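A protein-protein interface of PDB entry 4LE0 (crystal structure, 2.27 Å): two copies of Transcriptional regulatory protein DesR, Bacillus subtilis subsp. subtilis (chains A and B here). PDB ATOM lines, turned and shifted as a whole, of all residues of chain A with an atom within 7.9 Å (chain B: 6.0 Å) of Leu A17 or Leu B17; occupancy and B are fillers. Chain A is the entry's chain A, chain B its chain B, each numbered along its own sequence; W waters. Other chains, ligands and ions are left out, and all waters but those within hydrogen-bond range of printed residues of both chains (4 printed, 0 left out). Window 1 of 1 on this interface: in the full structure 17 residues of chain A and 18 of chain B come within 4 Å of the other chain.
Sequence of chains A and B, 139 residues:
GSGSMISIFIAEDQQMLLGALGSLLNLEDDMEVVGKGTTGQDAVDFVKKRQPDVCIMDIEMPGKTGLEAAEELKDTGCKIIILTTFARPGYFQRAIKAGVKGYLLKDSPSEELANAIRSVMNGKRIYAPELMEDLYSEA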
ATOM      1  N   ILE A  10      19.706   4.761  10.007  1.00  0.00           N
ATOM      2  CA  ILE A  10      20.811   4.666  10.963  1.00  0.00           C
ATOM      3  C   ILE A  10      21.630   3.429  10.686  1.00  0.00           C
ATOM      4  O   ILE A  10      21.091   2.331  10.781  1.00  0.00           O
ATOM      5  CB  ILE A  10      20.363   4.682  12.455  1.00  0.00           C
ATOM      6  CG1 ILE A  10      19.213   5.684  12.731  1.00  0.00           C
ATOM      7  CG2 ILE A  10      21.578   4.917  13.376  1.00  0.00           C
ATOM      8  CD1 ILE A  10      18.705   5.651  14.143  1.00  0.00           C
ATOM      9  N   GLU A  12      24.656   1.368  12.310  1.00  0.00           N
ATOM     10  CA  GLU A  12      25.417   1.189  13.544  1.00  0.00           C
ATOM     11  C   GLU A  12      25.444  -0.302  13.836  1.00  0.00           C
ATOM     12  O   GLU A  12      24.384  -0.913  13.935  1.00  0.00           O
ATOM     13  CB  GLU A  12      24.747   2.001  14.685  1.00  0.00           C
ATOM     14  CG  GLU A  12      25.259   1.719  16.086  1.00  0.00           C
ATOM     15  CD  GLU A  12      26.743   1.928  16.269  1.00  0.00           C
ATOM     16  OE1 GLU A  12      27.228   3.026  15.916  1.00  0.00           O
ATOM     17  OE2 GLU A  12      27.424   0.991  16.744  1.00  0.00           O
ATOM     18  N   ASP A  13      26.652  -0.904  13.926  1.00  0.00           N
ATOM     19  CA  ASP A  13      26.796  -2.351  14.133  1.00  0.00           C
ATOM     20  C   ASP A  13      26.420  -2.846  15.514  1.00  0.00           C
ATOM     21  O   ASP A  13      25.979  -3.983  15.638  1.00  0.00           O
ATOM     22  CB  ASP A  13      28.166  -2.873  13.694  1.00  0.00           C
ATOM     23  CG  ASP A  13      29.324  -2.389  14.510  1.00  0.00           C
ATOM     24  OD1 ASP A  13      29.492  -1.164  14.618  1.00  0.00           O
ATOM     25  OD2 ASP A  13      30.101  -3.243  15.007  1.00  0.00           O
ATOM     26  N   GLN A  14      26.581  -2.004  16.546  1.00  0.00           N
ATOM     27  CA  GLN A  14      26.238  -2.384  17.915  1.00  0.00           C
ATOM     28  C   GLN A  14      24.741  -2.149  18.091  1.00  0.00           C
ATOM     29  O   GLN A  14      24.298  -0.999  18.174  1.00  0.00           O
ATOM     30  CB  GLN A  14      27.070  -1.585  18.930  1.00  0.00           C
ATOM     31  CG  GLN A  14      28.582  -1.705  18.711  1.00  0.00           C
ATOM     32  CD  GLN A  14      29.306  -2.295  19.894  1.00  0.00           C
ATOM     33  OE1 GLN A  14      30.052  -1.603  20.594  1.00  0.00           O
ATOM     34  NE2 GLN A  14      29.203  -3.595  20.108  1.00  0.00           N
ATOM     35  N   GLN A  15      23.962  -3.256  18.055  1.00  0.00           N
ATOM     36  CA  GLN A  15      22.500  -3.317  18.122  1.00  0.00           C
ATOM     37  C   GLN A  15      21.879  -2.510  19.261  1.00  0.00           C
ATOM     38  O   GLN A  15      20.843  -1.897  19.045  1.00  0.00           O
ATOM     39  CB  GLN A  15      22.043  -4.770  18.233  1.00  0.00           C
ATOM     40  CG  GLN A  15      21.874  -5.480  16.909  1.00  0.00           C
ATOM     41  CD  GLN A  15      21.091  -6.745  17.139  1.00  0.00           C
ATOM     42  OE1 GLN A  15      21.653  -7.795  17.449  1.00  0.00           O
ATOM     43  NE2 GLN A  15      19.770  -6.651  17.098  1.00  0.00           N
ATOM     44  N   MET A  16      22.478  -2.554  20.475  1.00  0.00           N
ATOM     45  CA  MET A  16      22.022  -1.844  21.668  1.00  0.00           C
ATOM     46  C   MET A  16      22.030  -0.341  21.386  1.00  0.00           C
ATOM     47  O   MET A  16      21.024   0.337  21.604  1.00  0.00           O
ATOM     48  CB  MET A  16      22.930  -2.215  22.859  1.00  0.00           C
ATOM     49  CG  MET A  16      22.602  -1.546  24.188  1.00  0.00           C
ATOM     50  SD  MET A  16      21.036  -2.020  24.951  1.00  0.00           S
ATOM     51  CE  MET A  16      21.324  -3.812  25.268  1.00  0.00           C
ATOM     52  N   LEU A  17      23.131   0.144  20.805  1.00  0.00           N
ATOM     53  CA  LEU A  17      23.359   1.539  20.425  1.00  0.00           C
ATOM     54  C   LEU A  17      22.472   1.931  19.240  1.00  0.00           C
ATOM     55  O   LEU A  17      21.936   3.031  19.237  1.00  0.00           O
ATOM     56  CB  LEU A  17      24.847   1.712  20.067  1.00  0.00           C
ATOM     57  CG  LEU A  17      25.914   1.533  21.181  1.00  0.00           C
ATOM     58  CD1 LEU A  17      25.868   0.236  21.900  1.00  0.00           C
ATOM     59  CD2 LEU A  17      27.316   1.711  20.618  1.00  0.00           C
ATOM     60  N   LEU A  18      22.298   1.028  18.246  1.00  0.00           N
ATOM     61  CA  LEU A  18      21.450   1.245  17.064  1.00  0.00           C
ATOM     62  C   LEU A  18      19.984   1.486  17.492  1.00  0.00           C
ATOM     63  O   LEU A  18      19.361   2.463  17.059  1.00  0.00           O
ATOM     64  CB  LEU A  18      21.578   0.065  16.072  1.00  0.00           C
ATOM     65  CG  LEU A  18      20.619   0.053  14.859  1.00  0.00           C
ATOM     66  CD1 LEU A  18      20.892   1.198  13.909  1.00  0.00           C
ATOM     67  CD2 LEU A  18      20.712  -1.227  14.117  1.00  0.00           C
ATOM     68  N   GLY A  19      19.487   0.611  18.378  1.00  0.00           N
ATOM     69  CA  GLY A  19      18.150   0.684  18.958  1.00  0.00           C
ATOM     70  C   GLY A  19      17.972   1.930  19.796  1.00  0.00           C
ATOM     71  O   GLY A  19      16.980   2.633  19.627  1.00  0.00           O
ATOM     72  N   ALA A  20      18.974   2.264  20.639  1.00  0.00           N
ATOM     73  CA  ALA A  20      18.940   3.471  21.477  1.00  0.00           C
ATOM     74  C   ALA A  20      18.953   4.788  20.657  1.00  0.00           C
ATOM     75  O   ALA A  20      18.247   5.727  21.015  1.00  0.00           O
ATOM     76  CB  ALA A  20      20.065   3.442  22.518  1.00  0.00           C
ATOM     77  N   LEU A  21      19.701   4.826  19.539  1.00  0.00           N
ATOM     78  CA  LEU A  21      19.761   5.984  18.635  1.00  0.00           C
ATOM     79  C   LEU A  21      18.435   6.229  17.902  1.00  0.00           C
ATOM     80  O   LEU A  21      18.011   7.385  17.779  1.00  0.00           O
ATOM     81  CB  LEU A  21      20.938   5.886  17.647  1.00  0.00           C
ATOM     82  CG  LEU A  21      22.349   6.013  18.250  1.00  0.00           C
ATOM     83  CD1 LEU A  21      23.418   5.496  17.291  1.00  0.00           C
ATOM     84  CD2 LEU A  21      22.652   7.454  18.753  1.00  0.00           C
ATOM     85  N   GLY A  22      17.780   5.146  17.465  1.00  0.00           N
ATOM     86  CA  GLY A  22      16.471   5.198  16.809  1.00  0.00           C
ATOM     87  C   GLY A  22      15.429   5.768  17.752  1.00  0.00           C
ATOM     88  O   GLY A  22      14.603   6.591  17.358  1.00  0.00           O
ATOM     89  N   SER A  23      15.505   5.354  19.027  1.00  0.00           N
ATOM     90  CA  SER A  23      14.654   5.793  20.129  1.00  0.00           C
ATOM     91  C   SER A  23      14.916   7.280  20.439  1.00  0.00           C
ATOM     92  O   SER A  23      13.976   8.025  20.681  1.00  0.00           O
ATOM     93  CB  SER A  23      14.918   4.915  21.352  1.00  0.00           C
ATOM     94  OG  SER A  23      14.627   5.571  22.568  1.00  0.00           O
ATOM     95  N   LEU A  24      16.188   7.700  20.436  1.00  0.00           N
ATOM     96  CA  LEU A  24      16.597   9.079  20.685  1.00  0.00           C
ATOM     97  C   LEU A  24      16.049  10.054  19.607  1.00  0.00           C
ATOM     98  O   LEU A  24      15.637  11.167  19.946  1.00  0.00           O
ATOM     99  CB  LEU A  24      18.133   9.145  20.798  1.00  0.00           C
ATOM    100  CG  LEU A  24      18.796  10.516  20.993  1.00  0.00           C
ATOM    101  CD1 LEU A  24      18.526  11.088  22.384  1.00  0.00           C
ATOM    102  CD2 LEU A  24      20.283  10.448  20.698  1.00  0.00           C
ATOM    103  N   LYS A  36      16.971   0.907   9.757  1.00  0.00           N
ATOM    104  CA  LYS A  36      18.119   0.661  10.627  1.00  0.00           C
ATOM    105  C   LYS A  36      18.980  -0.449  10.027  1.00  0.00           C
ATOM    106  O   LYS A  36      18.449  -1.415   9.465  1.00  0.00           O
ATOM    107  CB  LYS A  36      17.641   0.273  12.035  1.00  0.00           C
ATOM    108  CG  LYS A  36      17.195   1.477  12.875  1.00  0.00           C
ATOM    109  CD  LYS A  36      16.853   1.097  14.302  1.00  0.00           C
ATOM    110  CE  LYS A  36      15.502   0.445  14.437  1.00  0.00           C
ATOM    111  NZ  LYS A  36      15.218   0.073  15.855  1.00  0.00           N
ATOM    112  N   ASP A  58      27.865   5.100  11.240  1.00  0.00           N
ATOM    113  CA  ASP A  58      28.968   4.664  12.078  1.00  0.00           C
ATOM    114  C   ASP A  58      30.144   4.359  11.120  1.00  0.00           C
ATOM    115  O   ASP A  58      29.899   4.068   9.953  1.00  0.00           O
ATOM    116  CB  ASP A  58      28.565   3.396  12.820  1.00  0.00           C
ATOM    117  CG  ASP A  58      29.622   2.815  13.723  1.00  0.00           C
ATOM    118  OD1 ASP A  58      30.384   3.605  14.345  1.00  0.00           O
ATOM    119  OD2 ASP A  58      29.667   1.593  13.850  1.00  0.00           O
ATOM    120  N   LEU A  83      28.745   9.324  12.677  1.00  0.00           N
ATOM    121  CA  LEU A  83      28.638   9.286  14.133  1.00  0.00           C
ATOM    122  C   LEU A  83      29.534   8.142  14.561  1.00  0.00           C
ATOM    123  O   LEU A  83      29.237   6.985  14.282  1.00  0.00           O
ATOM    124  CB  LEU A  83      27.184   9.133  14.633  1.00  0.00           C
ATOM    125  CG  LEU A  83      27.026   9.033  16.173  1.00  0.00           C
ATOM    126  CD1 LEU A  83      27.608  10.274  16.904  1.00  0.00           C
ATOM    127  CD2 LEU A  83      25.576   8.754  16.567  1.00  0.00           C
ATOM    128  N   THR A  85      33.077   6.743  17.407  1.00  0.00           N
ATOM    129  CA  THR A  85      33.933   6.810  18.602  1.00  0.00           C
ATOM    130  C   THR A  85      35.253   7.521  18.198  1.00  0.00           C
ATOM    131  O   THR A  85      35.863   8.209  19.014  1.00  0.00           O
ATOM    132  CB  THR A  85      34.251   5.356  19.060  1.00  0.00           C
ATOM    133  OG1 THR A  85      33.060   4.744  19.535  1.00  0.00           O
ATOM    134  CG2 THR A  85      35.301   5.278  20.163  1.00  0.00           C
ATOM    135  N   LEU A 105      30.953  12.951  17.123  1.00  0.00           N
ATOM    136  CA  LEU A 105      31.585  11.928  17.954  1.00  0.00           C
ATOM    137  C   LEU A 105      30.557  11.329  18.899  1.00  0.00           C
ATOM    138  O   LEU A 105      29.584  11.996  19.256  1.00  0.00           O
ATOM    139  CB  LEU A 105      32.806  12.482  18.732  1.00  0.00           C
ATOM    140  CG  LEU A 105      34.055  12.838  17.905  1.00  0.00           C
ATOM    141  CD1 LEU A 105      35.111  13.474  18.783  1.00  0.00           C
ATOM    142  CD2 LEU A 105      34.657  11.612  17.205  1.00  0.00           C
ATOM    143  N   LYS A 106      30.769  10.079  19.313  1.00  0.00           N
ATOM    144  CA  LYS A 106      29.873   9.416  20.271  1.00  0.00           C
ATOM    145  C   LYS A 106      30.065  10.044  21.689  1.00  0.00           C
ATOM    146  O   LYS A 106      29.344   9.729  22.620  1.00  0.00           O
ATOM    147  CB  LYS A 106      30.064   7.881  20.236  1.00  0.00           C
ATOM    148  CG  LYS A 106      29.341   7.250  19.055  1.00  0.00           C
ATOM    149  CD  LYS A 106      29.620   5.774  18.935  1.00  0.00           C
ATOM    150  CE  LYS A 106      29.026   5.200  17.668  1.00  0.00           C
ATOM    151  NZ  LYS A 106      29.379   3.761  17.506  1.00  0.00           N
ATOM    152  N   ASP A 107      31.024  10.953  21.820  1.00  0.00           N
ATOM    153  CA  ASP A 107      31.240  11.706  23.044  1.00  0.00           C
ATOM    154  C   ASP A 107      30.635  13.128  22.951  1.00  0.00           C
ATOM    155  O   ASP A 107      30.811  13.934  23.853  1.00  0.00           O
ATOM    156  CB  ASP A 107      32.718  11.737  23.456  1.00  0.00           C
ATOM    157  CG  ASP A 107      32.895  11.407  24.922  1.00  0.00           C
ATOM    158  OD1 ASP A 107      32.142  11.991  25.773  1.00  0.00           O
ATOM    159  OD2 ASP A 107      33.738  10.541  25.229  1.00  0.00           O
ATOM    160  N   SER A 108      29.915  13.417  21.869  1.00  0.00           N
ATOM    161  CA  SER A 108      29.204  14.687  21.714  1.00  0.00           C
ATOM    162  C   SER A 108      27.912  14.553  22.537  1.00  0.00           C
ATOM    163  O   SER A 108      27.372  13.443  22.598  1.00  0.00           O
ATOM    164  CB  SER A 108      28.813  14.912  20.251  1.00  0.00           C
ATOM    165  OG  SER A 108      29.917  15.017  19.365  1.00  0.00           O
ATOM    166  N   PRO A 109      27.360  15.634  23.132  1.00  0.00           N
ATOM    167  CA  PRO A 109      26.081  15.482  23.860  1.00  0.00           C
ATOM    168  C   PRO A 109      25.008  14.918  22.932  1.00  0.00           C
ATOM    169  O   PRO A 109      25.040  15.219  21.738  1.00  0.00           O
ATOM    170  CB  PRO A 109      25.749  16.917  24.302  1.00  0.00           C
ATOM    171  CG  PRO A 109      27.053  17.611  24.327  1.00  0.00           C
ATOM    172  CD  PRO A 109      27.839  17.031  23.188  1.00  0.00           C
ATOM    173  N   SER A 110      24.099  14.070  23.455  1.00  0.00           N
ATOM    174  CA  SER A 110      23.040  13.428  22.648  1.00  0.00           C
ATOM    175  C   SER A 110      22.133  14.414  21.893  1.00  0.00           C
ATOM    176  O   SER A 110      21.738  14.118  20.763  1.00  0.00           O
ATOM    177  CB  SER A 110      22.209  12.460  23.486  1.00  0.00           C
ATOM    178  OG  SER A 110      21.685  13.103  24.635  1.00  0.00           O
ATOM    179  N   GLU B  12      27.837   5.803  31.810  1.00  0.00           N
ATOM    180  CA  GLU B  12      28.348   5.581  30.457  1.00  0.00           C
ATOM    181  C   GLU B  12      29.123   6.830  30.067  1.00  0.00           C
ATOM    182  O   GLU B  12      28.562   7.919  30.104  1.00  0.00           O
ATOM    183  CB  GLU B  12      27.152   5.278  29.490  1.00  0.00           C
ATOM    184  CG  GLU B  12      27.470   5.302  28.002  1.00  0.00           C
ATOM    185  CD  GLU B  12      28.556   4.340  27.578  1.00  0.00           C
ATOM    186  OE1 GLU B  12      28.422   3.140  27.914  1.00  0.00           O
ATOM    187  OE2 GLU B  12      29.546   4.777  26.940  1.00  0.00           O
ATOM    188  N   GLN B  14      30.472   7.745  27.101  1.00  0.00           N
ATOM    189  CA  GLN B  14      30.149   8.312  25.797  1.00  0.00           C
ATOM    190  C   GLN B  14      28.761   8.930  25.903  1.00  0.00           C
ATOM    191  O   GLN B  14      27.768   8.205  25.960  1.00  0.00           O
ATOM    192  CB  GLN B  14      30.246   7.243  24.697  1.00  0.00           C
ATOM    193  CG  GLN B  14      31.582   6.477  24.651  1.00  0.00           C
ATOM    194  CD  GLN B  14      32.766   7.291  24.196  1.00  0.00           C
ATOM    195  OE1 GLN B  14      33.672   7.593  24.982  1.00  0.00           O
ATOM    196  NE2 GLN B  14      32.742   7.715  22.944  1.00  0.00           N
ATOM    197  N   GLN B  15      28.721  10.273  25.999  1.00  0.00           N
ATOM    198  CA  GLN B  15      27.544  11.131  26.186  1.00  0.00           C
ATOM    199  C   GLN B  15      26.402  10.846  25.229  1.00  0.00           C
ATOM    200  O   GLN B  15      25.250  10.894  25.653  1.00  0.00           O
ATOM    201  CB  GLN B  15      27.928  12.606  26.063  1.00  0.00           C
ATOM    202  CG  GLN B  15      28.457  13.242  27.318  1.00  0.00           C
ATOM    203  CD  GLN B  15      28.535  14.728  27.098  1.00  0.00           C
ATOM    204  OE1 GLN B  15      29.545  15.259  26.614  1.00  0.00           O
ATOM    205  NE2 GLN B  15      27.430  15.417  27.358  1.00  0.00           N
ATOM    206  N   MET B  16      26.716  10.597  23.939  1.00  0.00           N
ATOM    207  CA  MET B  16      25.741  10.309  22.895  1.00  0.00           C
ATOM    208  C   MET B  16      24.979   9.040  23.256  1.00  0.00           C
ATOM    209  O   MET B  16      23.751   9.036  23.264  1.00  0.00           O
ATOM    210  CB  MET B  16      26.453  10.193  21.526  1.00  0.00           C
ATOM    211  CG  MET B  16      25.527   9.938  20.332  1.00  0.00           C
ATOM    212  SD  MET B  16      24.338  11.266  19.982  1.00  0.00           S
ATOM    213  CE  MET B  16      25.442  12.639  19.481  1.00  0.00           C
ATOM    214  N   LEU B  17      25.721   8.000  23.639  1.00  0.00           N
ATOM    215  CA  LEU B  17      25.221   6.688  24.063  1.00  0.00           C
ATOM    216  C   LEU B  17      24.495   6.772  25.402  1.00  0.00           C
ATOM    217  O   LEU B  17      23.463   6.124  25.566  1.00  0.00           O
ATOM    218  CB  LEU B  17      26.398   5.693  24.143  1.00  0.00           C
ATOM    219  CG  LEU B  17      27.250   5.481  22.850  1.00  0.00           C
ATOM    220  CD1 LEU B  17      28.342   4.539  23.066  1.00  0.00           C
ATOM    221  CD2 LEU B  17      26.401   5.286  21.547  1.00  0.00           C
ATOM    222  N   LEU B  18      25.018   7.582  26.356  1.00  0.00           N
ATOM    223  CA  LEU B  18      24.411   7.803  27.676  1.00  0.00           C
ATOM    224  C   LEU B  18      22.994   8.419  27.514  1.00  0.00           C
ATOM    225  O   LEU B  18      22.026   7.925  28.104  1.00  0.00           O
ATOM    226  CB  LEU B  18      25.333   8.674  28.567  1.00  0.00           C
ATOM    227  CG  LEU B  18      24.763   9.158  29.906  1.00  0.00           C
ATOM    228  CD1 LEU B  18      24.557   8.027  30.867  1.00  0.00           C
ATOM    229  CD2 LEU B  18      25.654  10.174  30.531  1.00  0.00           C
ATOM    230  N   GLY B  19      22.906   9.454  26.686  1.00  0.00           N
ATOM    231  CA  GLY B  19      21.664  10.147  26.358  1.00  0.00           C
ATOM    232  C   GLY B  19      20.692   9.243  25.631  1.00  0.00           C
ATOM    233  O   GLY B  19      19.515   9.207  25.990  1.00  0.00           O
ATOM    234  N   ALA B  20      21.188   8.455  24.646  1.00  0.00           N
ATOM    235  CA  ALA B  20      20.353   7.516  23.885  1.00  0.00           C
ATOM    236  C   ALA B  20      19.799   6.365  24.762  1.00  0.00           C
ATOM    237  O   ALA B  20      18.650   5.984  24.582  1.00  0.00           O
ATOM    238  CB  ALA B  20      21.110   6.979  22.672  1.00  0.00           C
ATOM    239  N   LEU B  21      20.586   5.871  25.742  1.00  0.00           N
ATOM    240  CA  LEU B  21      20.167   4.828  26.692  1.00  0.00           C
ATOM    241  C   LEU B  21      19.072   5.311  27.637  1.00  0.00           C
ATOM    242  O   LEU B  21      18.119   4.573  27.881  1.00  0.00           O
ATOM    243  CB  LEU B  21      21.357   4.235  27.467  1.00  0.00           C
ATOM    244  CG  LEU B  21      22.344   3.372  26.661  1.00  0.00           C
ATOM    245  CD1 LEU B  21      23.673   3.192  27.409  1.00  0.00           C
ATOM    246  CD2 LEU B  21      21.727   2.018  26.246  1.00  0.00           C
ATOM    247  N   GLY B  22      19.198   6.545  28.129  1.00  0.00           N
ATOM    248  CA  GLY B  22      18.206   7.170  29.002  1.00  0.00           C
ATOM    249  C   GLY B  22      16.875   7.322  28.282  1.00  0.00           C
ATOM    250  O   GLY B  22      15.816   7.061  28.851  1.00  0.00           O
ATOM    251  N   LYS B 106      26.963  -4.518  24.398  1.00  0.00           N
ATOM    252  CA  LYS B 106      26.426  -3.426  23.575  1.00  0.00           C
ATOM    253  C   LYS B 106      25.982  -3.960  22.194  1.00  0.00           C
ATOM    254  O   LYS B 106      25.376  -3.238  21.396  1.00  0.00           O
ATOM    255  CB  LYS B 106      27.433  -2.271  23.485  1.00  0.00           C
ATOM    256  CG  LYS B 106      27.411  -1.399  24.733  1.00  0.00           C
ATOM    257  CD  LYS B 106      28.458  -0.316  24.688  1.00  0.00           C
ATOM    258  CE  LYS B 106      28.516   0.436  25.988  1.00  0.00           C
ATOM    259  NZ  LYS B 106      29.613   1.449  25.990  1.00  0.00           N
ATOM    260  N   ASP B 107      26.266  -5.251  21.936  1.00  0.00           N
ATOM    261  CA  ASP B 107      25.824  -5.905  20.725  1.00  0.00           C
ATOM    262  C   ASP B 107      24.579  -6.762  20.963  1.00  0.00           C
ATOM    263  O   ASP B 107      24.130  -7.458  20.059  1.00  0.00           O
ATOM    264  CB  ASP B 107      26.961  -6.660  20.025  1.00  0.00           C
ATOM    265  CG  ASP B 107      27.013  -6.326  18.536  1.00  0.00           C
ATOM    266  OD1 ASP B 107      25.927  -6.382  17.861  1.00  0.00           O
ATOM    267  OD2 ASP B 107      28.116  -5.972  18.043  1.00  0.00           O
ATOM    268  N   SER B 108      23.999  -6.678  22.173  1.00  0.00           N
ATOM    269  CA  SER B 108      22.747  -7.355  22.532  1.00  0.00           C
ATOM    270  C   SER B 108      21.626  -6.513  21.919  1.00  0.00           C
ATOM    271  O   SER B 108      21.769  -5.290  21.874  1.00  0.00           O
ATOM    272  CB  SER B 108      22.556  -7.371  24.053  1.00  0.00           C
ATOM    273  OG  SER B 108      23.541  -8.114  24.757  1.00  0.00           O
ATOM    274  N   SER B 110      18.556  -4.024  21.627  1.00  0.00           N
ATOM    275  CA  SER B 110      18.148  -2.965  22.566  1.00  0.00           C
ATOM    276  C   SER B 110      17.043  -3.382  23.565  1.00  0.00           C
ATOM    277  O   SER B 110      17.081  -2.943  24.712  1.00  0.00           O
ATOM    278  CB  SER B 110      17.749  -1.695  21.821  1.00  0.00           C
ATOM    279  OG  SER B 110      16.704  -1.954  20.897  1.00  0.00           O
HETATM  280  O   HOH W   1      29.723  -5.671  22.169  1.00  0.00           O
HETATM  281  O   HOH W   2      31.870  16.305  24.463  1.00  0.00           O
HETATM  282  O   HOH W   3      33.908   9.455  20.892  1.00  0.00           O
HETATM  283  O   HOH W   4      34.971   9.375  27.194  1.00  0.00           O
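OD2 of Asp B107 sits at hydrogen-bond distance from NE2 of Gln A14, 3.3 Å away.
The backbone NH (N) of Met A16 sits close to the backbone carbonyl oxygen (O) of Lys B106, 3.1 Å away.
The backbone carbonyl oxygen of Ser B108 lies within hydrogen-bond range of the backbone NH of Met A16, at 3.2 Å.
The backbone carbonyl oxygen (O) of Lys A106 is in hydrogen-bond range of the backbone NH (N) of Gln B15 (3.5 Å).
The backbone carbonyl oxygen of Lys A106 lies within hydrogen-bond range of the backbone NH of Met B16 (3.1 Å).
OD2 of Asp A107 lies close to OE1 of Gln B14 (3.0 Å).
The backbone carbonyl oxygen (O) of Asp A107 sits close to the side-chain amide oxygen (OE1) of Gln B15.
O of Ser A108 is in hydrogen-bond range of N of Met B16 (3.2 Å).
O of Asp A13 sits close to OD1 of Asp B107, 3.3 Å away.
The side-chain carboxylate (OE2) of Glu A12 sits at hydrogen-bond distance from the backbone NH (N) of Gln A14 (3.1 Å).
The side-chain amino group (NZ) of Lys A106 is in salt-bridge range of the side-chain carboxylate (OE1) of Glu A12 (2.8 Å).
OD1 of Asp A58 sits close to NZ of Lys A106, 3.3 Å away.
The side-chain hydroxyl of Ser A108 sits at hydrogen-bond distance from the backbone carbonyl oxygen of Leu A105 (3.0 Å).
The side-chain carboxylate (OE2) of Glu B12 sits at hydrogen-bond distance from the backbone NH (N) of Gln B14.
OE1 of Glu B12 lies within salt-bridge range of NZ of Lys B106 (2.8 Å).
Among the printed residues, pairs that only touch across the chains: Leu A17 with Lys B106 (3.4 Å), Lys A106 with Gln B14 (3.4 Å), Gln A14 with Lys B106 (3.4 Å), Ser A110 with Gly B19 (3.4 Å), Pro A109 with Met B16 (3.5 Å), Ala A20 with Ala B20 (3.5 Å), Gly A19 with Ser B110 (3.6 Å), Ser A108 with Gln B15 (3.6 Å), Gln A15 with Asp B107 (3.6 Å), Gln A15 with Lys B106 (3.6 Å), Ser A110 with Met B16 (3.7 Å), Gln A15 with Ser B108 (3.7 Å), Pro A109 with Gln B15 (3.7 Å), Leu A17 with Leu B17 (3.8 Å), Met A16 with Ser B110 (3.9 Å) and Leu A83 with Met B16 (3.9 Å).
Of the printed residues of chain B, Leu A17 touches Leu B17 and Lys B106.
Of the printed residues of chain A, Leu B17 touches Leu A17 (3.8 Å).
Of the printed residues of chain A, Met B16 touches Leu A83, Lys A106, Ser A108, Pro A109 and Ser A110.
Of the printed residues of chain B, Met A16 touches Lys B106, Ser B108 and Ser B110.
Printed residues of chain A within 4 Å of Asp B107: Asp A13 (3.3 Å), Gln A14 (3.3 Å) and Gln A15 (3.6 Å).
Glu B12 touches none of the printed residues of chain A.
Leu A18 touches none of the printed residues of chain B.
The nearest residue of chain B that does not touch Leu A17 is Ala B20 (5.3 Å).
Of the 14 printed residues of chain B, 10 touch a printed residue of chain A.
Printed residues of chain B that touch a printed residue of chain A: Gln B14, Gln B15, Met B16, Leu B17, Gly B19, Ala B20, Lys B106, Asp B107, Ser B108 and Ser B110.
Hydrophobic or aromatic side chains of chain B within 4 Å of the printed part of chain A: Met B16, Leu B17 and Ala B20.
Of the 24 printed residues of chain A, 13 touch a printed residue of chain B.
Printed residues of chain A that touch a printed residue of chain B: Asp A13, Gln A14, Gln A15, Met A16, Leu A17, Gly A19, Ala A20, Leu A83, Lys A106, Asp A107, Ser A108, Pro A109 and Ser A110.
Among the printed residues, 25 pairs touch across the chains.
Among the printed residues, no Asp or Glu carboxylate lies within 4 Å of a Lys or Arg side-chain nitrogen of the other chain.
Gln A15 touches Ser B108, and with the chains exchanged Ser A108 touches Gln B15.
Met A16 touches Ser B108, and with the chains exchanged Ser A108 touches Met B16.
Leu A17 touches Lys B106, but with the chains exchanged Lys A106 does not touch Leu B17 (4.1 Å).
Gly A19 touches Ser B110, and with the chains exchanged Ser A110 touches Gly B19.
Positions printed for both chains: 12, 14, 15, 16, 17, 18, 19, 20, 21, 22, 106, 107, 108 and 110.
Water W4 lies within hydrogen-bond range of OD2 of Asp A107 (2.6 Å) and OE1 of Gln B14 (3.1 Å).
Water W2 lies within hydrogen-bond range of the backbone carbonyl oxygen of Asp A107 (2.7 Å) and the side-chain amide oxygen of Gln B15 (3.3 Å).
Water W3 lies within hydrogen-bond range of NE2 of Gln B14, O of Thr A85 and N of Asp A107.
Water W1 bridges the side-chain amide nitrogen (NE2) of Gln A14 (3.0 Å) and the backbone NH (N) of Asp B107 (3.5 Å).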
